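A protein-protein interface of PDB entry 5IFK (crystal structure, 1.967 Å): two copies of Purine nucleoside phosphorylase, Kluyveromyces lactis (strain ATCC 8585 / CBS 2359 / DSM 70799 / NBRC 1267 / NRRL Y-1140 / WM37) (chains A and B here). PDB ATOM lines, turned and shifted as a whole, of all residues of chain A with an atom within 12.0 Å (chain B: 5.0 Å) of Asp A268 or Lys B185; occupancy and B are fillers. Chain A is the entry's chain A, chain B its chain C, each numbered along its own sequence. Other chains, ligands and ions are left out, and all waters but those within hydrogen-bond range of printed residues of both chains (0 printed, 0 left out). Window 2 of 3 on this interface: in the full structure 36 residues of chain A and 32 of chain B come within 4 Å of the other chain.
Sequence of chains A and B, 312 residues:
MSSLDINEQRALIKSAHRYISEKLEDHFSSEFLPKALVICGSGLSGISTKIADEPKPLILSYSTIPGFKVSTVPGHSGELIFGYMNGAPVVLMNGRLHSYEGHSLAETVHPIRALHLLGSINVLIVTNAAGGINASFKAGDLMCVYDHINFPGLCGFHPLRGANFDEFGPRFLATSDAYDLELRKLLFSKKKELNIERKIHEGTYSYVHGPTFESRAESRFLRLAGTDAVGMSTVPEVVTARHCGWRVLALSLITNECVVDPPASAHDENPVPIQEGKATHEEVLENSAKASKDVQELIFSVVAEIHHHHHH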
ATOM      1  N   ARG A 216     -28.140  30.779 -27.640  1.00  0.00           N
ATOM      2  CA  ARG A 216     -27.761  31.020 -29.033  1.00  0.00           C
ATOM      3  C   ARG A 216     -28.597  30.172 -30.003  1.00  0.00           C
ATOM      4  O   ARG A 216     -29.094  30.662 -31.013  1.00  0.00           O
ATOM      5  CB  ARG A 216     -26.283  30.735 -29.221  1.00  0.00           C
ATOM      6  CG  ARG A 216     -25.405  31.542 -28.301  1.00  0.00           C
ATOM      7  CD  ARG A 216     -24.191  30.711 -27.928  1.00  0.00           C
ATOM      8  NE  ARG A 216     -23.294  31.442 -27.048  1.00  0.00           N
ATOM      9  CZ  ARG A 216     -22.354  32.275 -27.474  1.00  0.00           C
ATOM     10  NH1 ARG A 216     -22.183  32.480 -28.774  1.00  0.00           N
ATOM     11  NH2 ARG A 216     -21.587  32.901 -26.592  1.00  0.00           N
ATOM     12  N   ASP A 261     -24.458  33.305 -32.813  1.00  0.00           N
ATOM     13  CA  ASP A 261     -23.331  32.465 -33.217  1.00  0.00           C
ATOM     14  C   ASP A 261     -23.166  31.306 -32.250  1.00  0.00           C
ATOM     15  O   ASP A 261     -23.412  31.460 -31.054  1.00  0.00           O
ATOM     16  CB  ASP A 261     -22.030  33.262 -33.277  1.00  0.00           C
ATOM     17  CG  ASP A 261     -21.998  34.241 -34.425  1.00  0.00           C
ATOM     18  OD1 ASP A 261     -22.782  34.077 -35.388  1.00  0.00           O
ATOM     19  OD2 ASP A 261     -21.174  35.175 -34.355  1.00  0.00           O
ATOM     20  N   PRO A 262     -22.739  30.144 -32.766  1.00  0.00           N
ATOM     21  CA  PRO A 262     -22.514  28.979 -31.905  1.00  0.00           C
ATOM     22  C   PRO A 262     -21.507  29.322 -30.826  1.00  0.00           C
ATOM     23  O   PRO A 262     -20.603  30.117 -31.081  1.00  0.00           O
ATOM     24  CB  PRO A 262     -21.947  27.927 -32.865  1.00  0.00           C
ATOM     25  CG  PRO A 262     -22.347  28.393 -34.230  1.00  0.00           C
ATOM     26  CD  PRO A 262     -22.357  29.881 -34.163  1.00  0.00           C
ATOM     27  N   PRO A 263     -21.655  28.742 -29.629  1.00  0.00           N
ATOM     28  CA  PRO A 263     -20.614  28.986 -28.623  1.00  0.00           C
ATOM     29  C   PRO A 263     -19.276  28.364 -29.021  1.00  0.00           C
ATOM     30  O   PRO A 263     -19.221  27.482 -29.880  1.00  0.00           O
ATOM     31  CB  PRO A 263     -21.183  28.332 -27.353  1.00  0.00           C
ATOM     32  CG  PRO A 263     -22.156  27.329 -27.837  1.00  0.00           C
ATOM     33  CD  PRO A 263     -22.720  27.849 -29.140  1.00  0.00           C
ATOM     34  N   ALA A 264     -18.207  28.846 -28.402  1.00  0.00           N
ATOM     35  CA  ALA A 264     -16.870  28.324 -28.635  1.00  0.00           C
ATOM     36  C   ALA A 264     -16.845  26.808 -28.488  1.00  0.00           C
ATOM     37  O   ALA A 264     -17.417  26.253 -27.555  1.00  0.00           O
ATOM     38  CB  ALA A 264     -15.892  28.961 -27.681  1.00  0.00           C
ATOM     39  N   SER A 265     -16.213  26.145 -29.443  1.00  0.00           N
ATOM     40  CA  SER A 265     -15.968  24.719 -29.349  1.00  0.00           C
ATOM     41  C   SER A 265     -14.837  24.415 -28.382  1.00  0.00           C
ATOM     42  O   SER A 265     -13.837  25.152 -28.305  1.00  0.00           O
ATOM     43  CB  SER A 265     -15.630  24.143 -30.723  1.00  0.00           C
ATOM     44  OG  SER A 265     -14.988  22.889 -30.591  1.00  0.00           O
ATOM     45  N   ALA A 266     -14.972  23.306 -27.664  1.00  0.00           N
ATOM     46  CA  ALA A 266     -13.880  22.808 -26.848  1.00  0.00           C
ATOM     47  C   ALA A 266     -12.606  22.528 -27.674  1.00  0.00           C
ATOM     48  O   ALA A 266     -11.529  22.407 -27.116  1.00  0.00           O
ATOM     49  CB  ALA A 266     -14.312  21.550 -26.099  1.00  0.00           C
ATOM     50  N   HIS A 267     -12.722  22.427 -28.995  1.00  0.00           N
ATOM     51  CA  HIS A 267     -11.544  22.157 -29.818  1.00  0.00           C
ATOM     52  C   HIS A 267     -10.933  23.425 -30.426  1.00  0.00           C
ATOM     53  O   HIS A 267      -9.940  23.341 -31.142  1.00  0.00           O
ATOM     54  CB  HIS A 267     -11.904  21.172 -30.928  1.00  0.00           C
ATOM     55  CG  HIS A 267     -12.622  19.956 -30.431  1.00  0.00           C
ATOM     56  ND1 HIS A 267     -13.955  19.722 -30.688  1.00  0.00           N
ATOM     57  CD2 HIS A 267     -12.198  18.919 -29.672  1.00  0.00           C
ATOM     58  CE1 HIS A 267     -14.322  18.592 -30.109  1.00  0.00           C
ATOM     59  NE2 HIS A 267     -13.273  18.085 -29.487  1.00  0.00           N
ATOM     60  N   ASP A 268     -11.538  24.583 -30.161  1.00  0.00           N
ATOM     61  CA  ASP A 268     -11.009  25.859 -30.649  1.00  0.00           C
ATOM     62  C   ASP A 268      -9.730  26.234 -29.904  1.00  0.00           C
ATOM     63  O   ASP A 268      -9.682  26.162 -28.679  1.00  0.00           O
ATOM     64  CB  ASP A 268     -12.049  26.978 -30.492  1.00  0.00           C
ATOM     65  CG  ASP A 268     -13.286  26.763 -31.356  1.00  0.00           C
ATOM     66  OD1 ASP A 268     -13.179  26.057 -32.385  1.00  0.00           O
ATOM     67  OD2 ASP A 268     -14.366  27.306 -31.007  1.00  0.00           O
ATOM     68  N   GLU A 269      -8.687  26.631 -30.624  1.00  0.00           N
ATOM     69  CA  GLU A 269      -7.458  27.020 -29.940  1.00  0.00           C
ATOM     70  C   GLU A 269      -7.581  28.438 -29.385  1.00  0.00           C
ATOM     71  O   GLU A 269      -6.986  28.768 -28.355  1.00  0.00           O
ATOM     72  CB  GLU A 269      -6.240  26.904 -30.862  1.00  0.00           C
ATOM     73  CG  GLU A 269      -6.512  27.074 -32.351  1.00  0.00           C
ATOM     74  CD  GLU A 269      -5.233  27.008 -33.186  1.00  0.00           C
ATOM     75  OE1 GLU A 269      -4.433  27.974 -33.144  1.00  0.00           O
ATOM     76  OE2 GLU A 269      -5.015  25.974 -33.858  1.00  0.00           O
ATOM     77  N   ASN A 270      -8.362  29.271 -30.062  1.00  0.00           N
ATOM     78  CA  ASN A 270      -8.607  30.629 -29.599  1.00  0.00           C
ATOM     79  C   ASN A 270     -10.097  30.902 -29.441  1.00  0.00           C
ATOM     80  O   ASN A 270     -10.682  31.658 -30.218  1.00  0.00           O
ATOM     81  CB  ASN A 270      -7.991  31.644 -30.560  1.00  0.00           C
ATOM     82  CG  ASN A 270      -6.479  31.590 -30.574  1.00  0.00           C
ATOM     83  OD1 ASN A 270      -5.820  32.153 -29.700  1.00  0.00           O
ATOM     84  ND2 ASN A 270      -5.921  30.925 -31.575  1.00  0.00           N
ATOM     85  N   PRO A 271     -10.713  30.291 -28.419  1.00  0.00           N
ATOM     86  CA  PRO A 271     -12.159  30.373 -28.211  1.00  0.00           C
ATOM     87  C   PRO A 271     -12.632  31.755 -27.781  1.00  0.00           C
ATOM     88  O   PRO A 271     -11.937  32.483 -27.062  1.00  0.00           O
ATOM     89  CB  PRO A 271     -12.403  29.360 -27.099  1.00  0.00           C
ATOM     90  CG  PRO A 271     -11.142  29.373 -26.315  1.00  0.00           C
ATOM     91  CD  PRO A 271     -10.048  29.546 -27.335  1.00  0.00           C
ATOM     92  N   VAL A 272     -13.823  32.108 -28.242  1.00  0.00           N
ATOM     93  CA  VAL A 272     -14.497  33.327 -27.813  1.00  0.00           C
ATOM     94  C   VAL A 272     -15.297  33.031 -26.543  1.00  0.00           C
ATOM     95  O   VAL A 272     -16.092  32.093 -26.524  1.00  0.00           O
ATOM     96  CB  VAL A 272     -15.422  33.868 -28.926  1.00  0.00           C
ATOM     97  CG1 VAL A 272     -16.329  34.974 -28.397  1.00  0.00           C
ATOM     98  CG2 VAL A 272     -14.588  34.364 -30.097  1.00  0.00           C
ATOM     99  N   PRO A 273     -15.067  33.815 -25.470  1.00  0.00           N
ATOM    100  CA  PRO A 273     -15.745  33.605 -24.180  1.00  0.00           C
ATOM    101  C   PRO A 273     -17.258  33.507 -24.339  1.00  0.00           C
ATOM    102  O   PRO A 273     -17.862  34.375 -24.959  1.00  0.00           O
ATOM    103  CB  PRO A 273     -15.368  34.847 -23.372  1.00  0.00           C
ATOM    104  CG  PRO A 273     -14.069  35.291 -23.956  1.00  0.00           C
ATOM    105  CD  PRO A 273     -14.109  34.936 -25.419  1.00  0.00           C
ATOM    106  N   ILE A 274     -17.860  32.463 -23.782  1.00  0.00           N
ATOM    107  CA  ILE A 274     -19.280  32.216 -24.021  1.00  0.00           C
ATOM    108  C   ILE A 274     -20.162  33.301 -23.402  1.00  0.00           C
ATOM    109  O   ILE A 274     -21.304  33.494 -23.813  1.00  0.00           O
ATOM    110  CB  ILE A 274     -19.710  30.831 -23.486  1.00  0.00           C
ATOM    111  CG1 ILE A 274     -19.443  30.724 -21.977  1.00  0.00           C
ATOM    112  CG2 ILE A 274     -18.998  29.722 -24.265  1.00  0.00           C
ATOM    113  CD1 ILE A 274     -20.015  29.471 -21.330  1.00  0.00           C
ATOM    114  N   GLU A 276     -19.390  36.453 -23.557  1.00  0.00           N
ATOM    115  CA  GLU A 276     -19.208  37.665 -24.350  1.00  0.00           C
ATOM    116  C   GLU A 276     -20.525  38.088 -25.018  1.00  0.00           C
ATOM    117  O   GLU A 276     -21.210  37.276 -25.665  1.00  0.00           O
ATOM    118  CB  GLU A 276     -18.108  37.461 -25.400  1.00  0.00           C
ATOM    119  CG  GLU A 276     -18.182  38.397 -26.615  1.00  0.00           C
ATOM    120  CD  GLU A 276     -18.938  37.791 -27.795  1.00  0.00           C
ATOM    121  OE1 GLU A 276     -19.037  36.545 -27.871  1.00  0.00           O
ATOM    122  OE2 GLU A 276     -19.435  38.566 -28.643  1.00  0.00           O
ATOM    123  N   LEU B 181     -17.185  26.344 -20.972  1.00  0.00           N
ATOM    124  CA  LEU B 181     -16.239  25.900 -21.993  1.00  0.00           C
ATOM    125  C   LEU B 181     -15.082  25.097 -21.398  1.00  0.00           C
ATOM    126  O   LEU B 181     -14.606  24.119 -21.992  1.00  0.00           O
ATOM    127  CB  LEU B 181     -15.686  27.105 -22.756  1.00  0.00           C
ATOM    128  CG  LEU B 181     -14.469  26.847 -23.648  1.00  0.00           C
ATOM    129  CD1 LEU B 181     -14.832  25.975 -24.846  1.00  0.00           C
ATOM    130  CD2 LEU B 181     -13.871  28.166 -24.100  1.00  0.00           C
ATOM    131  N   GLU B 182     -14.622  25.531 -20.228  1.00  0.00           N
ATOM    132  CA  GLU B 182     -13.491  24.888 -19.567  1.00  0.00           C
ATOM    133  C   GLU B 182     -13.840  23.446 -19.154  1.00  0.00           C
ATOM    134  O   GLU B 182     -13.026  22.524 -19.301  1.00  0.00           O
ATOM    135  CB  GLU B 182     -13.044  25.719 -18.357  1.00  0.00           C
ATOM    136  CG  GLU B 182     -12.318  27.036 -18.715  1.00  0.00           C
ATOM    137  CD  GLU B 182     -13.229  28.077 -19.382  1.00  0.00           C
ATOM    138  OE1 GLU B 182     -14.458  28.078 -19.117  1.00  0.00           O
ATOM    139  OE2 GLU B 182     -12.720  28.892 -20.182  1.00  0.00           O
ATOM    140  N   LEU B 183     -15.061  23.246 -18.663  1.00  0.00           N
ATOM    141  CA  LEU B 183     -15.505  21.901 -18.301  1.00  0.00           C
ATOM    142  C   LEU B 183     -15.593  21.018 -19.545  1.00  0.00           C
ATOM    143  O   LEU B 183     -15.254  19.828 -19.493  1.00  0.00           O
ATOM    144  CB  LEU B 183     -16.855  21.937 -17.568  1.00  0.00           C
ATOM    145  CG  LEU B 183     -16.875  22.606 -16.187  1.00  0.00           C
ATOM    146  CD1 LEU B 183     -18.249  22.455 -15.516  1.00  0.00           C
ATOM    147  CD2 LEU B 183     -15.764  22.068 -15.287  1.00  0.00           C
ATOM    148  N   ARG B 184     -16.023  21.595 -20.667  1.00  0.00           N
ATOM    149  CA  ARG B 184     -16.085  20.822 -21.906  1.00  0.00           C
ATOM    150  C   ARG B 184     -14.680  20.452 -22.377  1.00  0.00           C
ATOM    151  O   ARG B 184     -14.458  19.336 -22.840  1.00  0.00           O
ATOM    152  CB  ARG B 184     -16.838  21.587 -22.989  1.00  0.00           C
ATOM    153  CG  ARG B 184     -18.334  21.662 -22.695  1.00  0.00           C
ATOM    154  CD  ARG B 184     -19.129  22.297 -23.842  1.00  0.00           C
ATOM    155  NE  ARG B 184     -19.069  23.751 -23.815  1.00  0.00           N
ATOM    156  CZ  ARG B 184     -18.540  24.494 -24.780  1.00  0.00           C
ATOM    157  NH1 ARG B 184     -18.002  23.925 -25.854  1.00  0.00           N
ATOM    158  NH2 ARG B 184     -18.553  25.809 -24.667  1.00  0.00           N
ATOM    159  N   LYS B 185     -13.735  21.378 -22.244  1.00  0.00           N
ATOM    160  CA  LYS B 185     -12.346  21.086 -22.588  1.00  0.00           C
ATOM    161  C   LYS B 185     -11.758  20.027 -21.650  1.00  0.00           C
ATOM    162  O   LYS B 185     -10.994  19.157 -22.075  1.00  0.00           O
ATOM    163  CB  LYS B 185     -11.494  22.359 -22.546  1.00  0.00           C
ATOM    164  CG  LYS B 185     -11.687  23.278 -23.746  1.00  0.00           C
ATOM    165  CD  LYS B 185     -10.757  24.494 -23.661  1.00  0.00           C
ATOM    166  CE  LYS B 185     -10.958  25.429 -24.839  1.00  0.00           C
ATOM    167  NZ  LYS B 185     -10.548  24.836 -26.144  1.00  0.00           N
ATOM    168  N   LEU B 186     -12.114  20.105 -20.373  1.00  0.00           N
ATOM    169  CA  LEU B 186     -11.708  19.091 -19.411  1.00  0.00           C
ATOM    170  C   LEU B 186     -12.214  17.709 -19.828  1.00  0.00           C
ATOM    171  O   LEU B 186     -11.477  16.721 -19.771  1.00  0.00           O
ATOM    172  CB  LEU B 186     -12.222  19.443 -18.016  1.00  0.00           C
ATOM    173  CG  LEU B 186     -12.077  18.384 -16.923  1.00  0.00           C
ATOM    174  CD1 LEU B 186     -10.609  17.950 -16.738  1.00  0.00           C
ATOM    175  CD2 LEU B 186     -12.634  18.919 -15.614  1.00  0.00           C
ATOM    176  N   LEU B 187     -13.471  17.642 -20.255  1.00  0.00           N
ATOM    177  CA  LEU B 187     -14.054  16.372 -20.664  1.00  0.00           C
ATOM    178  C   LEU B 187     -13.304  15.754 -21.842  1.00  0.00           C
ATOM    179  O   LEU B 187     -13.032  14.558 -21.841  1.00  0.00           O
ATOM    180  CB  LEU B 187     -15.536  16.541 -21.029  1.00  0.00           C
ATOM    181  CG  LEU B 187     -16.209  15.350 -21.722  1.00  0.00           C
ATOM    182  CD1 LEU B 187     -16.341  14.143 -20.789  1.00  0.00           C
ATOM    183  CD2 LEU B 187     -17.575  15.762 -22.249  1.00  0.00           C
ATOM    184  N   PHE B 188     -12.976  16.560 -22.850  1.00  0.00           N
ATOM    185  CA  PHE B 188     -12.287  16.033 -24.020  1.00  0.00           C
ATOM    186  C   PHE B 188     -10.834  15.699 -23.739  1.00  0.00           C
ATOM    187  O   PHE B 188     -10.264  14.818 -24.383  1.00  0.00           O
ATOM    188  CB  PHE B 188     -12.386  17.018 -25.179  1.00  0.00           C
ATOM    189  CG  PHE B 188     -13.727  17.005 -25.839  1.00  0.00           C
ATOM    190  CD1 PHE B 188     -14.063  15.994 -26.719  1.00  0.00           C
ATOM    191  CD2 PHE B 188     -14.663  17.989 -25.553  1.00  0.00           C
ATOM    192  CE1 PHE B 188     -15.303  15.962 -27.316  1.00  0.00           C
ATOM    193  CE2 PHE B 188     -15.923  17.973 -26.152  1.00  0.00           C
ATOM    194  CZ  PHE B 188     -16.242  16.957 -27.034  1.00  0.00           C
ATOM    195  N   SER B 189     -10.232  16.385 -22.776  1.00  0.00           N
ATOM    196  CA  SER B 189      -8.871  16.035 -22.397  1.00  0.00           C
ATOM    197  C   SER B 189      -8.856  14.670 -21.703  1.00  0.00           C
ATOM    198  O   SER B 189      -7.908  13.908 -21.863  1.00  0.00           O
ATOM    199  CB  SER B 189      -8.250  17.109 -21.499  1.00  0.00           C
ATOM    200  OG  SER B 189      -8.897  17.161 -20.240  1.00  0.00           O
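Ala A264 touches Leu B181.
O of Ser A265 touches CD1 of Leu B181, 3.7 Å away.
NZ of Lys B185 touches O of Ser A265, 3.9 Å away.
CA of Ala A266 touches CD1 of Leu B181, 3.9 Å away.
N of Ala A266 touches NH1 of Arg B184 (3.6 Å).
Ala A266 touches Phe B188 (CB to CD2, 3.6 Å).
Phe B188 touches His A267 (CD1 to NE2, 3.6 Å).
Leu B181 touches Pro A271 (CD2 to CB, 3.5 Å).
Ile A274 touches Arg B184 (CG2 to NH2, 3.96 Å).
No position is printed for both chains.
Of the 9 printed residues of chain B, 4 touch a printed residue of chain A.
Hydrophobic or aromatic side chains of chain B that line the printed part of chain A: Leu B181 and Phe B188.
Printed residues of chain A that touch a printed residue of chain B: Ala A264, Ser A265, Ala A266, His A267, Asp A268, Pro A271 and Ile A274.
Of chain B, only Lys B185 comes within 4 Å of Asp A268.
Of chain A, only Ser A265, Ala A266 and Asp A268 come within 4 Å of Lys B185.
Of chain A, only Ala A264 (3.8 Å), Ser A265 (3.7 Å), Ala A266 (3.9 Å) and Pro A271 (3.5 Å) come within 4 Å of Leu B181.
Of chain A, only Ala A264 (2.9 Å), Ala A266 (3.6 Å) and Ile A274 (3.96 Å) come within 4 Å of Arg B184.
No residue of chain A comes within 4 Å of Leu B186.
No residue of chain A comes within 4 Å of Leu B187.
Of chain A, only Ala A266 (3.6 Å) and His A267 (3.6 Å) come within 4 Å of Phe B188.
No residue of chain A comes within 4 Å of Ser B189.
Of the printed residues of chain B, Pro A271 touches Leu B181.
Printed residues of chain B within 4 Å of Ala A264: Leu B181 and Arg B184.
Of the printed residues of chain B, Ala A266 touches Leu B181 (3.9 Å), Arg B184 (3.6 Å), Lys B185 (2.8 Å) and Phe B188 (3.6 Å).
Leu B183 touches none of the printed residues of chain A.
The nearest residue of chain A that does not touch Lys B185 is Pro A271 (4.2 Å).
The nearest printed residue of chain B that does not touch Ala A266 is Leu B186 (6.3 Å).
The backbone carbonyl oxygen of Asp A268 is in hydrogen-bond range of the side-chain amino group of Lys B185 (3.0 Å).
O of Ala A264 is in hydrogen-bond range of NH1 of Arg B184 (2.9 Å).
O of Ala A266 is in hydrogen-bond range of NZ of Lys B185 (2.8 Å).
The guanidinium group (NH2) of Arg A216 lies within hydrogen-bond range of the backbone carbonyl oxygen (O) of Ile A274 (2.9 Å).
The side-chain hydroxyl (OG) of Ser A265 sits at hydrogen-bond distance from the backbone NH (N) of His A267, at 2.8 Å.
N of Ser A265 lies within hydrogen-bond range of OD2 of Asp A268.
The side-chain hydroxyl (OG) of Ser B189 lies within hydrogen-bond range of the backbone carbonyl oxygen (O) of Lys B185 (3.4 Å).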
